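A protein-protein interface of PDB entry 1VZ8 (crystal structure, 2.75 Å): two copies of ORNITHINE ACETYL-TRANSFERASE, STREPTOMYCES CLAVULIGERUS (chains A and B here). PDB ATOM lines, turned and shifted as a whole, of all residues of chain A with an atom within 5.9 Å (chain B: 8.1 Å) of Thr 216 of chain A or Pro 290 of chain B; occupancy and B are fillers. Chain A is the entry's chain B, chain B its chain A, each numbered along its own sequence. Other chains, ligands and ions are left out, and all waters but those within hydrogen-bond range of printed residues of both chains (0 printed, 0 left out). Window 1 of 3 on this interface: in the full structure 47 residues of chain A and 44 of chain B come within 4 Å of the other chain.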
ATOM      1  N   LEU A 175     -11.511  28.530 -36.840  1.00  0.00           N
ATOM      2  CA  LEU A 175     -11.968  28.915 -38.160  1.00  0.00           C
ATOM      3  C   LEU A 175     -13.376  29.490 -38.351  1.00  0.00           C
ATOM      4  O   LEU A 175     -14.381  28.863 -38.006  1.00  0.00           O
ATOM      5  CB  LEU A 175     -11.785  27.693 -39.061  1.00  0.00           C
ATOM      6  CG  LEU A 175     -11.807  27.854 -40.569  1.00  0.00           C
ATOM      7  CD1 LEU A 175     -11.004  26.730 -41.200  1.00  0.00           C
ATOM      8  CD2 LEU A 175     -13.250  27.859 -41.058  1.00  0.00           C
ATOM      9  N   GLU A 176     -13.404  30.691 -38.924  1.00  0.00           N
ATOM     10  CA  GLU A 176     -14.599  31.464 -39.274  1.00  0.00           C
ATOM     11  C   GLU A 176     -14.034  32.744 -39.886  1.00  0.00           C
ATOM     12  O   GLU A 176     -14.064  33.814 -39.278  1.00  0.00           O
ATOM     13  CB  GLU A 176     -15.484  31.808 -38.062  1.00  0.00           C
ATOM     14  CG  GLU A 176     -16.518  32.920 -38.406  1.00  0.00           C
ATOM     15  CD  GLU A 176     -17.761  32.970 -37.506  1.00  0.00           C
ATOM     16  OE1 GLU A 176     -17.613  33.084 -36.259  1.00  0.00           O
ATOM     17  OE2 GLU A 176     -18.890  32.913 -38.067  1.00  0.00           O
ATOM     18  N   SER A 213     -18.070  28.414 -40.754  1.00  0.00           N
ATOM     19  CA  SER A 213     -17.580  28.584 -39.402  1.00  0.00           C
ATOM     20  C   SER A 213     -17.710  27.289 -38.608  1.00  0.00           C
ATOM     21  O   SER A 213     -18.808  26.739 -38.464  1.00  0.00           O
ATOM     22  CB  SER A 213     -18.361  29.710 -38.720  1.00  0.00           C
ATOM     23  OG  SER A 213     -18.175  29.703 -37.315  1.00  0.00           O
ATOM     24  N   ILE A 214     -16.576  26.798 -38.110  1.00  0.00           N
ATOM     25  CA  ILE A 214     -16.540  25.577 -37.307  1.00  0.00           C
ATOM     26  C   ILE A 214     -16.746  25.945 -35.826  1.00  0.00           C
ATOM     27  O   ILE A 214     -17.710  25.487 -35.184  1.00  0.00           O
ATOM     28  CB  ILE A 214     -15.171  24.853 -37.424  1.00  0.00           C
ATOM     29  CG1 ILE A 214     -14.814  24.600 -38.888  1.00  0.00           C
ATOM     30  CG2 ILE A 214     -15.210  23.537 -36.655  1.00  0.00           C
ATOM     31  CD1 ILE A 214     -15.681  23.575 -39.590  1.00  0.00           C
ATOM     32  N   ASP A 215     -15.847  26.794 -35.310  1.00  0.00           N
ATOM     33  CA  ASP A 215     -15.854  27.224 -33.905  1.00  0.00           C
ATOM     34  C   ASP A 215     -15.946  28.738 -33.618  1.00  0.00           C
ATOM     35  O   ASP A 215     -15.768  29.166 -32.473  1.00  0.00           O
ATOM     36  CB  ASP A 215     -14.595  26.696 -33.219  1.00  0.00           C
ATOM     37  CG  ASP A 215     -13.325  27.134 -33.932  1.00  0.00           C
ATOM     38  OD1 ASP A 215     -13.292  28.265 -34.485  1.00  0.00           O
ATOM     39  OD2 ASP A 215     -12.353  26.343 -33.929  1.00  0.00           O
ATOM     40  N   THR A 216     -16.213  29.537 -34.645  1.00  0.00           N
ATOM     41  CA  THR A 216     -16.316  30.994 -34.511  1.00  0.00           C
ATOM     42  C   THR A 216     -15.003  31.681 -34.157  1.00  0.00           C
ATOM     43  O   THR A 216     -14.973  32.906 -34.049  1.00  0.00           O
ATOM     44  CB  THR A 216     -17.300  31.462 -33.400  1.00  0.00           C
ATOM     45  OG1 THR A 216     -16.570  31.604 -32.170  1.00  0.00           O
ATOM     46  CG2 THR A 216     -18.478  30.490 -33.219  1.00  0.00           C
ATOM     47  N   ASP A 217     -13.923  30.926 -33.975  1.00  0.00           N
ATOM     48  CA  ASP A 217     -12.644  31.550 -33.588  1.00  0.00           C
ATOM     49  C   ASP A 217     -11.770  32.126 -34.702  1.00  0.00           C
ATOM     50  O   ASP A 217     -10.752  31.531 -35.067  1.00  0.00           O
ATOM     51  CB  ASP A 217     -11.799  30.573 -32.772  1.00  0.00           C
ATOM     52  CG  ASP A 217     -12.308  30.409 -31.365  1.00  0.00           C
ATOM     53  OD1 ASP A 217     -12.845  31.389 -30.821  1.00  0.00           O
ATOM     54  OD2 ASP A 217     -12.161  29.311 -30.796  1.00  0.00           O
ATOM     55  N   THR A 218     -12.148  33.296 -35.213  1.00  0.00           N
ATOM     56  CA  THR A 218     -11.402  33.944 -36.279  1.00  0.00           C
ATOM     57  C   THR A 218      -9.908  34.074 -36.020  1.00  0.00           C
ATOM     58  O   THR A 218      -9.458  34.830 -35.149  1.00  0.00           O
ATOM     59  CB  THR A 218     -11.990  35.301 -36.570  1.00  0.00           C
ATOM     60  OG1 THR A 218     -13.327  35.107 -37.003  1.00  0.00           O
ATOM     61  CG2 THR A 218     -11.222  36.018 -37.665  1.00  0.00           C
ATOM     62  N   ASN A 288     -23.661  28.759 -35.256  1.00  0.00           N
ATOM     63  CA  ASN A 288     -22.710  28.893 -34.129  1.00  0.00           C
ATOM     64  C   ASN A 288     -23.308  28.609 -32.739  1.00  0.00           C
ATOM     65  O   ASN A 288     -22.612  28.679 -31.720  1.00  0.00           O
ATOM     66  CB  ASN A 288     -22.038  30.280 -34.117  1.00  0.00           C
ATOM     67  CG  ASN A 288     -21.076  30.471 -35.278  1.00  0.00           C
ATOM     68  OD1 ASN A 288     -20.366  29.550 -35.661  1.00  0.00           O
ATOM     69  ND2 ASN A 288     -21.046  31.669 -35.835  1.00  0.00           N
ATOM     70  N   TYR A 384     -14.183  17.316 -30.556  1.00  0.00           N
ATOM     71  CA  TYR A 384     -13.640  18.677 -30.631  1.00  0.00           C
ATOM     72  C   TYR A 384     -13.106  19.134 -29.284  1.00  0.00           C
ATOM     73  O   TYR A 384     -12.043  19.748 -29.213  1.00  0.00           O
ATOM     74  CB  TYR A 384     -14.709  19.681 -31.104  1.00  0.00           C
ATOM     75  CG  TYR A 384     -14.235  21.135 -31.165  1.00  0.00           C
ATOM     76  CD1 TYR A 384     -14.071  21.893 -30.000  1.00  0.00           C
ATOM     77  CD2 TYR A 384     -13.939  21.739 -32.381  1.00  0.00           C
ATOM     78  CE1 TYR A 384     -13.625  23.208 -30.053  1.00  0.00           C
ATOM     79  CE2 TYR A 384     -13.499  23.049 -32.440  1.00  0.00           C
ATOM     80  CZ  TYR A 384     -13.344  23.773 -31.276  1.00  0.00           C
ATOM     81  OH  TYR A 384     -12.905  25.068 -31.346  1.00  0.00           O
ATOM     82  N   ASN A 388      -8.932  19.964 -28.820  1.00  0.00           N
ATOM     83  CA  ASN A 388      -8.547  21.303 -28.419  1.00  0.00           C
ATOM     84  C   ASN A 388      -8.344  21.447 -26.918  1.00  0.00           C
ATOM     85  O   ASN A 388      -8.066  22.536 -26.425  1.00  0.00           O
ATOM     86  CB  ASN A 388      -9.583  22.290 -28.924  1.00  0.00           C
ATOM     87  CG  ASN A 388      -9.616  22.346 -30.437  1.00  0.00           C
ATOM     88  OD1 ASN A 388      -8.609  22.667 -31.072  1.00  0.00           O
ATOM     89  ND2 ASN A 388     -10.767  22.030 -31.026  1.00  0.00           N
ATOM     90  N   THR B 216     -23.312  31.144 -24.664  1.00  0.00           N
ATOM     91  CA  THR B 216     -23.742  32.228 -25.563  1.00  0.00           C
ATOM     92  C   THR B 216     -25.165  32.119 -26.109  1.00  0.00           C
ATOM     93  O   THR B 216     -25.552  32.912 -26.970  1.00  0.00           O
ATOM     94  CB  THR B 216     -22.869  32.330 -26.824  1.00  0.00           C
ATOM     95  OG1 THR B 216     -23.268  31.309 -27.750  1.00  0.00           O
ATOM     96  CG2 THR B 216     -21.390  32.189 -26.493  1.00  0.00           C
ATOM     97  N   LYS B 284     -16.213  39.160 -22.926  1.00  0.00           N
ATOM     98  CA  LYS B 284     -17.073  38.068 -23.402  1.00  0.00           C
ATOM     99  C   LYS B 284     -16.424  37.276 -24.534  1.00  0.00           C
ATOM    100  O   LYS B 284     -16.439  36.042 -24.510  1.00  0.00           O
ATOM    101  CB  LYS B 284     -18.413  38.613 -23.891  1.00  0.00           C
ATOM    102  CG  LYS B 284     -19.372  39.086 -22.804  1.00  0.00           C
ATOM    103  CD  LYS B 284     -19.765  37.934 -21.895  1.00  0.00           C
ATOM    104  CE  LYS B 284     -20.946  38.315 -21.046  1.00  0.00           C
ATOM    105  NZ  LYS B 284     -21.959  39.025 -21.865  1.00  0.00           N
ATOM    106  N   THR B 285     -15.839  37.972 -25.513  1.00  0.00           N
ATOM    107  CA  THR B 285     -15.213  37.297 -26.649  1.00  0.00           C
ATOM    108  C   THR B 285     -14.238  36.247 -26.184  1.00  0.00           C
ATOM    109  O   THR B 285     -14.147  35.162 -26.764  1.00  0.00           O
ATOM    110  CB  THR B 285     -14.459  38.276 -27.563  1.00  0.00           C
ATOM    111  OG1 THR B 285     -15.394  39.141 -28.217  1.00  0.00           O
ATOM    112  CG2 THR B 285     -13.657  37.512 -28.617  1.00  0.00           C
ATOM    113  N   VAL B 286     -13.503  36.570 -25.130  1.00  0.00           N
ATOM    114  CA  VAL B 286     -12.532  35.634 -24.600  1.00  0.00           C
ATOM    115  C   VAL B 286     -13.266  34.457 -23.964  1.00  0.00           C
ATOM    116  O   VAL B 286     -13.052  33.311 -24.339  1.00  0.00           O
ATOM    117  CB  VAL B 286     -11.621  36.332 -23.548  1.00  0.00           C
ATOM    118  CG1 VAL B 286     -10.617  35.360 -22.961  1.00  0.00           C
ATOM    119  CG2 VAL B 286     -10.897  37.489 -24.189  1.00  0.00           C
ATOM    120  N   VAL B 287     -14.158  34.767 -23.026  1.00  0.00           N
ATOM    121  CA  VAL B 287     -14.900  33.763 -22.289  1.00  0.00           C
ATOM    122  C   VAL B 287     -15.749  32.824 -23.137  1.00  0.00           C
ATOM    123  O   VAL B 287     -15.935  31.644 -22.789  1.00  0.00           O
ATOM    124  CB  VAL B 287     -15.787  34.412 -21.232  1.00  0.00           C
ATOM    125  CG1 VAL B 287     -17.154  34.727 -21.816  1.00  0.00           C
ATOM    126  CG2 VAL B 287     -15.913  33.488 -20.054  1.00  0.00           C
ATOM    127  N   ASN B 288     -16.260  33.334 -24.252  1.00  0.00           N
ATOM    128  CA  ASN B 288     -17.090  32.517 -25.134  1.00  0.00           C
ATOM    129  C   ASN B 288     -16.307  31.759 -26.200  1.00  0.00           C
ATOM    130  O   ASN B 288     -16.843  30.841 -26.822  1.00  0.00           O
ATOM    131  CB  ASN B 288     -18.143  33.380 -25.816  1.00  0.00           C
ATOM    132  CG  ASN B 288     -19.086  34.027 -24.834  1.00  0.00           C
ATOM    133  OD1 ASN B 288     -19.489  33.410 -23.853  1.00  0.00           O
ATOM    134  ND2 ASN B 288     -19.460  35.279 -25.107  1.00  0.00           N
ATOM    135  N   SER B 289     -15.053  32.156 -26.422  1.00  0.00           N
ATOM    136  CA  SER B 289     -14.195  31.504 -27.408  1.00  0.00           C
ATOM    137  C   SER B 289     -14.095  30.017 -27.119  1.00  0.00           C
ATOM    138  O   SER B 289     -13.577  29.609 -26.082  1.00  0.00           O
ATOM    139  CB  SER B 289     -12.798  32.104 -27.370  1.00  0.00           C
ATOM    140  OG  SER B 289     -11.901  31.348 -28.170  1.00  0.00           O
ATOM    141  N   PRO B 290     -14.588  29.177 -28.026  1.00  0.00           N
ATOM    142  CA  PRO B 290     -14.478  27.745 -27.725  1.00  0.00           C
ATOM    143  C   PRO B 290     -13.022  27.297 -27.521  1.00  0.00           C
ATOM    144  O   PRO B 290     -12.731  26.436 -26.684  1.00  0.00           O
ATOM    145  CB  PRO B 290     -15.125  27.087 -28.936  1.00  0.00           C
ATOM    146  CG  PRO B 290     -16.132  28.111 -29.371  1.00  0.00           C
ATOM    147  CD  PRO B 290     -15.402  29.420 -29.227  1.00  0.00           C
ATOM    148  N   LEU B 291     -12.103  27.892 -28.277  1.00  0.00           N
ATOM    149  CA  LEU B 291     -10.696  27.517 -28.161  1.00  0.00           C
ATOM    150  C   LEU B 291     -10.067  27.920 -26.835  1.00  0.00           C
ATOM    151  O   LEU B 291      -9.072  27.325 -26.405  1.00  0.00           O
ATOM    152  CB  LEU B 291      -9.901  28.069 -29.339  1.00  0.00           C
ATOM    153  CG  LEU B 291     -10.218  27.219 -30.570  1.00  0.00           C
ATOM    154  CD1 LEU B 291      -9.478  27.762 -31.789  1.00  0.00           C
ATOM    155  CD2 LEU B 291      -9.831  25.760 -30.278  1.00  0.00           C
ATOM    156  N   VAL B 292     -10.656  28.922 -26.194  1.00  0.00           N
ATOM    157  CA  VAL B 292     -10.191  29.361 -24.899  1.00  0.00           C
ATOM    158  C   VAL B 292     -10.873  28.457 -23.879  1.00  0.00           C
ATOM    159  O   VAL B 292     -10.223  27.889 -23.018  1.00  0.00           O
ATOM    160  CB  VAL B 292     -10.576  30.835 -24.607  1.00  0.00           C
ATOM    161  CG1 VAL B 292     -10.179  31.205 -23.174  1.00  0.00           C
ATOM    162  CG2 VAL B 292      -9.865  31.759 -25.585  1.00  0.00           C
ATOM    163  N   LYS B 293     -12.186  28.308 -23.990  1.00  0.00           N
ATOM    164  CA  LYS B 293     -12.927  27.464 -23.059  1.00  0.00           C
ATOM    165  C   LYS B 293     -12.324  26.069 -22.938  1.00  0.00           C
ATOM    166  O   LYS B 293     -12.239  25.523 -21.837  1.00  0.00           O
ATOM    167  CB  LYS B 293     -14.376  27.321 -23.498  1.00  0.00           C
ATOM    168  CG  LYS B 293     -15.249  28.553 -23.328  1.00  0.00           C
ATOM    169  CD  LYS B 293     -16.490  28.394 -24.223  1.00  0.00           C
ATOM    170  CE  LYS B 293     -17.785  28.363 -23.440  1.00  0.00           C
ATOM    171  NZ  LYS B 293     -17.911  27.219 -22.519  1.00  0.00           N
ATOM    172  N   THR B 294     -11.914  25.490 -24.068  1.00  0.00           N
ATOM    173  CA  THR B 294     -11.337  24.150 -24.057  1.00  0.00           C
ATOM    174  C   THR B 294      -9.917  24.136 -23.530  1.00  0.00           C
ATOM    175  O   THR B 294      -9.494  23.159 -22.912  1.00  0.00           O
ATOM    176  CB  THR B 294     -11.362  23.487 -25.460  1.00  0.00           C
ATOM    177  OG1 THR B 294     -10.865  24.401 -26.442  1.00  0.00           O
ATOM    178  CG2 THR B 294     -12.766  23.078 -25.810  1.00  0.00           C
ATOM    179  N   ALA B 295      -9.174  25.209 -23.770  1.00  0.00           N
ATOM    180  CA  ALA B 295      -7.805  25.263 -23.273  1.00  0.00           C
ATOM    181  C   ALA B 295      -7.860  25.174 -21.749  1.00  0.00           C
ATOM    182  O   ALA B 295      -7.199  24.330 -21.148  1.00  0.00           O
ATOM    183  CB  ALA B 295      -7.123  26.559 -23.719  1.00  0.00           C
ATOM    184  N   VAL B 296      -8.672  26.039 -21.139  1.00  0.00           N
ATOM    185  CA  VAL B 296      -8.842  26.087 -19.687  1.00  0.00           C
ATOM    186  C   VAL B 296      -9.233  24.724 -19.157  1.00  0.00           C
ATOM    187  O   VAL B 296      -8.716  24.258 -18.123  1.00  0.00           O
ATOM    188  CB  VAL B 296      -9.929  27.098 -19.295  1.00  0.00           C
ATOM    189  CG1 VAL B 296     -10.289  26.946 -17.817  1.00  0.00           C
ATOM    190  CG2 VAL B 296      -9.425  28.520 -19.569  1.00  0.00           C
ATOM    191  N   HIS B 297     -10.152  24.089 -19.875  1.00  0.00           N
ATOM    192  CA  HIS B 297     -10.618  22.769 -19.514  1.00  0.00           C
ATOM    193  C   HIS B 297      -9.445  21.793 -19.436  1.00  0.00           C
ATOM    194  O   HIS B 297      -9.425  20.907 -18.588  1.00  0.00           O
ATOM    195  CB  HIS B 297     -11.623  22.257 -20.537  1.00  0.00           C
ATOM    196  CG  HIS B 297     -11.967  20.815 -20.343  1.00  0.00           C
ATOM    197  ND1 HIS B 297     -12.771  20.377 -19.313  1.00  0.00           N
ATOM    198  CD2 HIS B 297     -11.494  19.703 -20.950  1.00  0.00           C
ATOM    199  CE1 HIS B 297     -12.771  19.059 -19.288  1.00  0.00           C
ATOM    200  NE2 HIS B 297     -12.001  18.626 -20.270  1.00  0.00           N
ATOM    201  N   ARG B 305      -4.295  31.518 -27.495  1.00  0.00           N
ATOM    202  CA  ARG B 305      -5.716  31.486 -27.804  1.00  0.00           C
ATOM    203  C   ARG B 305      -6.461  32.712 -27.254  1.00  0.00           C
ATOM    204  O   ARG B 305      -7.421  33.178 -27.880  1.00  0.00           O
ATOM    205  CB  ARG B 305      -6.339  30.187 -27.288  1.00  0.00           C
ATOM    206  CG  ARG B 305      -5.852  28.978 -28.048  1.00  0.00           C
ATOM    207  CD  ARG B 305      -6.543  27.733 -27.601  1.00  0.00           C
ATOM    208  NE  ARG B 305      -6.084  26.550 -28.318  1.00  0.00           N
ATOM    209  CZ  ARG B 305      -6.454  25.312 -27.999  1.00  0.00           C
ATOM    210  NH1 ARG B 305      -7.282  25.102 -26.980  1.00  0.00           N
ATOM    211  NH2 ARG B 305      -6.004  24.283 -28.691  1.00  0.00           N
ATOM    212  N   MET B 308      -5.631  35.446 -29.804  1.00  0.00           N
ATOM    213  CA  MET B 308      -6.433  35.223 -30.993  1.00  0.00           C
ATOM    214  C   MET B 308      -7.819  35.734 -30.624  1.00  0.00           C
ATOM    215  O   MET B 308      -8.387  36.589 -31.314  1.00  0.00           O
ATOM    216  CB  MET B 308      -6.453  33.713 -31.316  1.00  0.00           C
ATOM    217  CG  MET B 308      -7.417  33.248 -32.424  1.00  0.00           C
ATOM    218  SD  MET B 308      -9.234  33.081 -31.778  1.00  0.00           S
ATOM    219  CE  MET B 308      -9.133  31.493 -30.680  1.00  0.00           C
ATOM    220  N   ALA B 309      -8.339  35.229 -29.512  1.00  0.00           N
ATOM    221  CA  ALA B 309      -9.647  35.637 -29.059  1.00  0.00           C
ATOM    222  C   ALA B 309      -9.733  37.143 -29.078  1.00  0.00           C
ATOM    223  O   ALA B 309     -10.553  37.710 -29.772  1.00  0.00           O
ATOM    224  CB  ALA B 309      -9.901  35.129 -27.662  1.00  0.00           C
ATOM    225  N   LYS B 312     -10.222  39.075 -32.228  1.00  0.00           N
ATOM    226  CA  LYS B 312     -11.477  38.910 -32.914  1.00  0.00           C
ATOM    227  C   LYS B 312     -12.232  40.206 -32.870  1.00  0.00           C
ATOM    228  O   LYS B 312     -13.043  40.490 -33.754  1.00  0.00           O
ATOM    229  CB  LYS B 312     -12.289  37.785 -32.275  1.00  0.00           C
ATOM    230  CG  LYS B 312     -11.532  36.479 -32.233  1.00  0.00           C
ATOM    231  CD  LYS B 312     -12.422  35.278 -32.510  1.00  0.00           C
ATOM    232  CE  LYS B 312     -13.503  35.099 -31.468  1.00  0.00           C
ATOM    233  NZ  LYS B 312     -13.937  33.665 -31.415  1.00  0.00           N
ATOM    234  N   CYS B 378     -17.241  29.633 -18.126  1.00  0.00           N
ATOM    235  CA  CYS B 378     -16.731  28.334 -17.738  1.00  0.00           C
ATOM    236  C   CYS B 378     -16.088  27.606 -18.919  1.00  0.00           C
ATOM    237  O   CYS B 378     -16.182  28.016 -20.074  1.00  0.00           O
ATOM    238  CB  CYS B 378     -17.850  27.488 -17.147  1.00  0.00           C
ATOM    239  SG  CYS B 378     -19.088  26.910 -18.359  1.00  0.00           S
ATOM    240  N   ASP B 379     -15.417  26.513 -18.603  1.00  0.00           N
ATOM    241  CA  ASP B 379     -14.747  25.730 -19.613  1.00  0.00           C
ATOM    242  C   ASP B 379     -15.787  24.968 -20.412  1.00  0.00           C
ATOM    243  O   ASP B 379     -16.975  24.993 -20.075  1.00  0.00           O
ATOM    244  CB  ASP B 379     -13.747  24.775 -18.937  1.00  0.00           C
ATOM    245  CG  ASP B 379     -14.384  23.911 -17.849  1.00  0.00           C
ATOM    246  OD1 ASP B 379     -15.476  24.272 -17.353  1.00  0.00           O
ATOM    247  OD2 ASP B 379     -13.784  22.873 -17.479  1.00  0.00           O
ATOM    248  N   LEU B 380     -15.343  24.330 -21.489  1.00  0.00           N
ATOM    249  CA  LEU B 380     -16.217  23.528 -22.328  1.00  0.00           C
ATOM    250  C   LEU B 380     -15.735  22.088 -22.171  1.00  0.00           C
ATOM    251  O   LEU B 380     -14.629  21.725 -22.573  1.00  0.00           O
ATOM    252  CB  LEU B 380     -16.127  23.980 -23.784  1.00  0.00           C
ATOM    253  CG  LEU B 380     -16.727  23.007 -24.807  1.00  0.00           C
ATOM    254  CD1 LEU B 380     -18.230  22.977 -24.671  1.00  0.00           C
ATOM    255  CD2 LEU B 380     -16.304  23.408 -26.216  1.00  0.00           C
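OG of Ser 289 of chain B is in hydrogen-bond range of OD1 of Asp 217 of chain A. N of Leu 291 of chain B sits close to OD2 of Asp 217 of chain A (2.9 Å). The backbone carbonyl oxygen (O) of Asn 388 of chain A lies within hydrogen-bond range of the side-chain hydroxyl (OG1) of Thr 294 of chain B, at 3.4 Å. NH1 of Arg 305 of chain B sits at hydrogen-bond distance from O of Asn 388 of chain A. NZ of Lys 312 of chain B sits at hydrogen-bond distance from O of Thr 216 of chain A, at 2.9 Å. The side-chain carboxylate (OD1) of Asp 217 of chain A is in salt-bridge range of the side-chain amino group (NZ) of Lys 312 of chain B (2.6 Å).
Printed residues of chain B that touch a printed residue of chain A: Ser 289, Pro 290, Leu 291, Thr 294, Ala 295, Arg 305, Met 308 and Lys 312. Hydrophobic or aromatic side chains of chain B that line the printed part of chain A: Pro 290, Leu 291 and Met 308. Along chain B the printed residues that touch a printed residue of chain A span positions 289 to 312.
Of chain A, only Asp 215 (3.3 Å), Thr 216 (3.8 Å), Asp 217 (3.6 Å) and Tyr 384 (3.8 Å) come within 4 Å of Pro 290 of chain B. Of the printed residues of chain B, Asp 217 of chain A touches Ser 289, Pro 290, Leu 291, Met 308 and Lys 312. Of the printed residues of chain A, Lys 312 of chain B touches Thr 216, Asp 217 and Thr 218. Of the printed residues of chain A, Ser 289 of chain B touches Asp 217 (2.8 Å). Printed residues of chain B within 4 Å of Asp 215 of chain A: Pro 290 (3.3 Å) and Leu 291 (3.9 Å). Of the printed residues of chain A, Thr 294 of chain B touches Asn 388. Val 286 of chain B touches none of the printed residues of chain A. The nearest residue of chain A that does not touch Pro 290 of chain B is Asn 388 of chain A (5.7 Å). The nearest printed residue of chain B that does not touch Thr 218 of chain A is Ala 309 of chain B (5.8 Å).
OG of Ser 289 of chain B lies close to N of Leu 291 of chain B, 3.5 Å away. The side-chain hydroxyl of Ser 289 of chain B lies close to the backbone NH of Val 292 of chain B (3.4 Å). O of Leu 291 of chain B is in hydrogen-bond range of OG1 of Thr 294 of chain B (3.4 Å). The side-chain hydroxyl (OG1) of Thr 218 of chain A sits at hydrogen-bond distance from the backbone carbonyl oxygen (O) of Glu 176 of chain A, 2.7 Å away. The side-chain carboxylate (OD2) of Asp 215 of chain A lies within hydrogen-bond range of the side-chain hydroxyl (OH) of Tyr 384 of chain A, at 2.9 Å. The side-chain amide nitrogen (ND2) of Asn 388 of chain A lies close to the backbone carbonyl oxygen (O) of Tyr 384 of chain A (3.2 Å).
Leu 291 of chain B touches Asp 215 of chain A (CD1 to OD2, 3.9 Å). OG1 of Thr 216 of chain A touches CD of Pro 290 of chain B, at 3.8 Å. CD of Pro 290 of chain B touches OD1 of Asp 217 of chain A, at 3.6 Å. Asp 217 of chain A touches Met 308 of chain B (CG to CE, 3.4 Å). Thr 218 of chain A touches Met 308 of chain B (O to CG, 3.8 Å). Lys 312 of chain B touches Thr 218 of chain A (CD to N, 3.4 Å). Tyr 384 of chain A touches Pro 290 of chain B (OH to CB, 3.8 Å). OH of Tyr 384 of chain A touches CD2 of Leu 291 of chain B, at 3.3 Å. Leu 291 of chain B touches Asn 388 of chain A (CD2 to OD1, 3.4 Å). Ala 295 of chain B touches Asn 388 of chain A.
Positions printed for both chains: 216 and 288.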
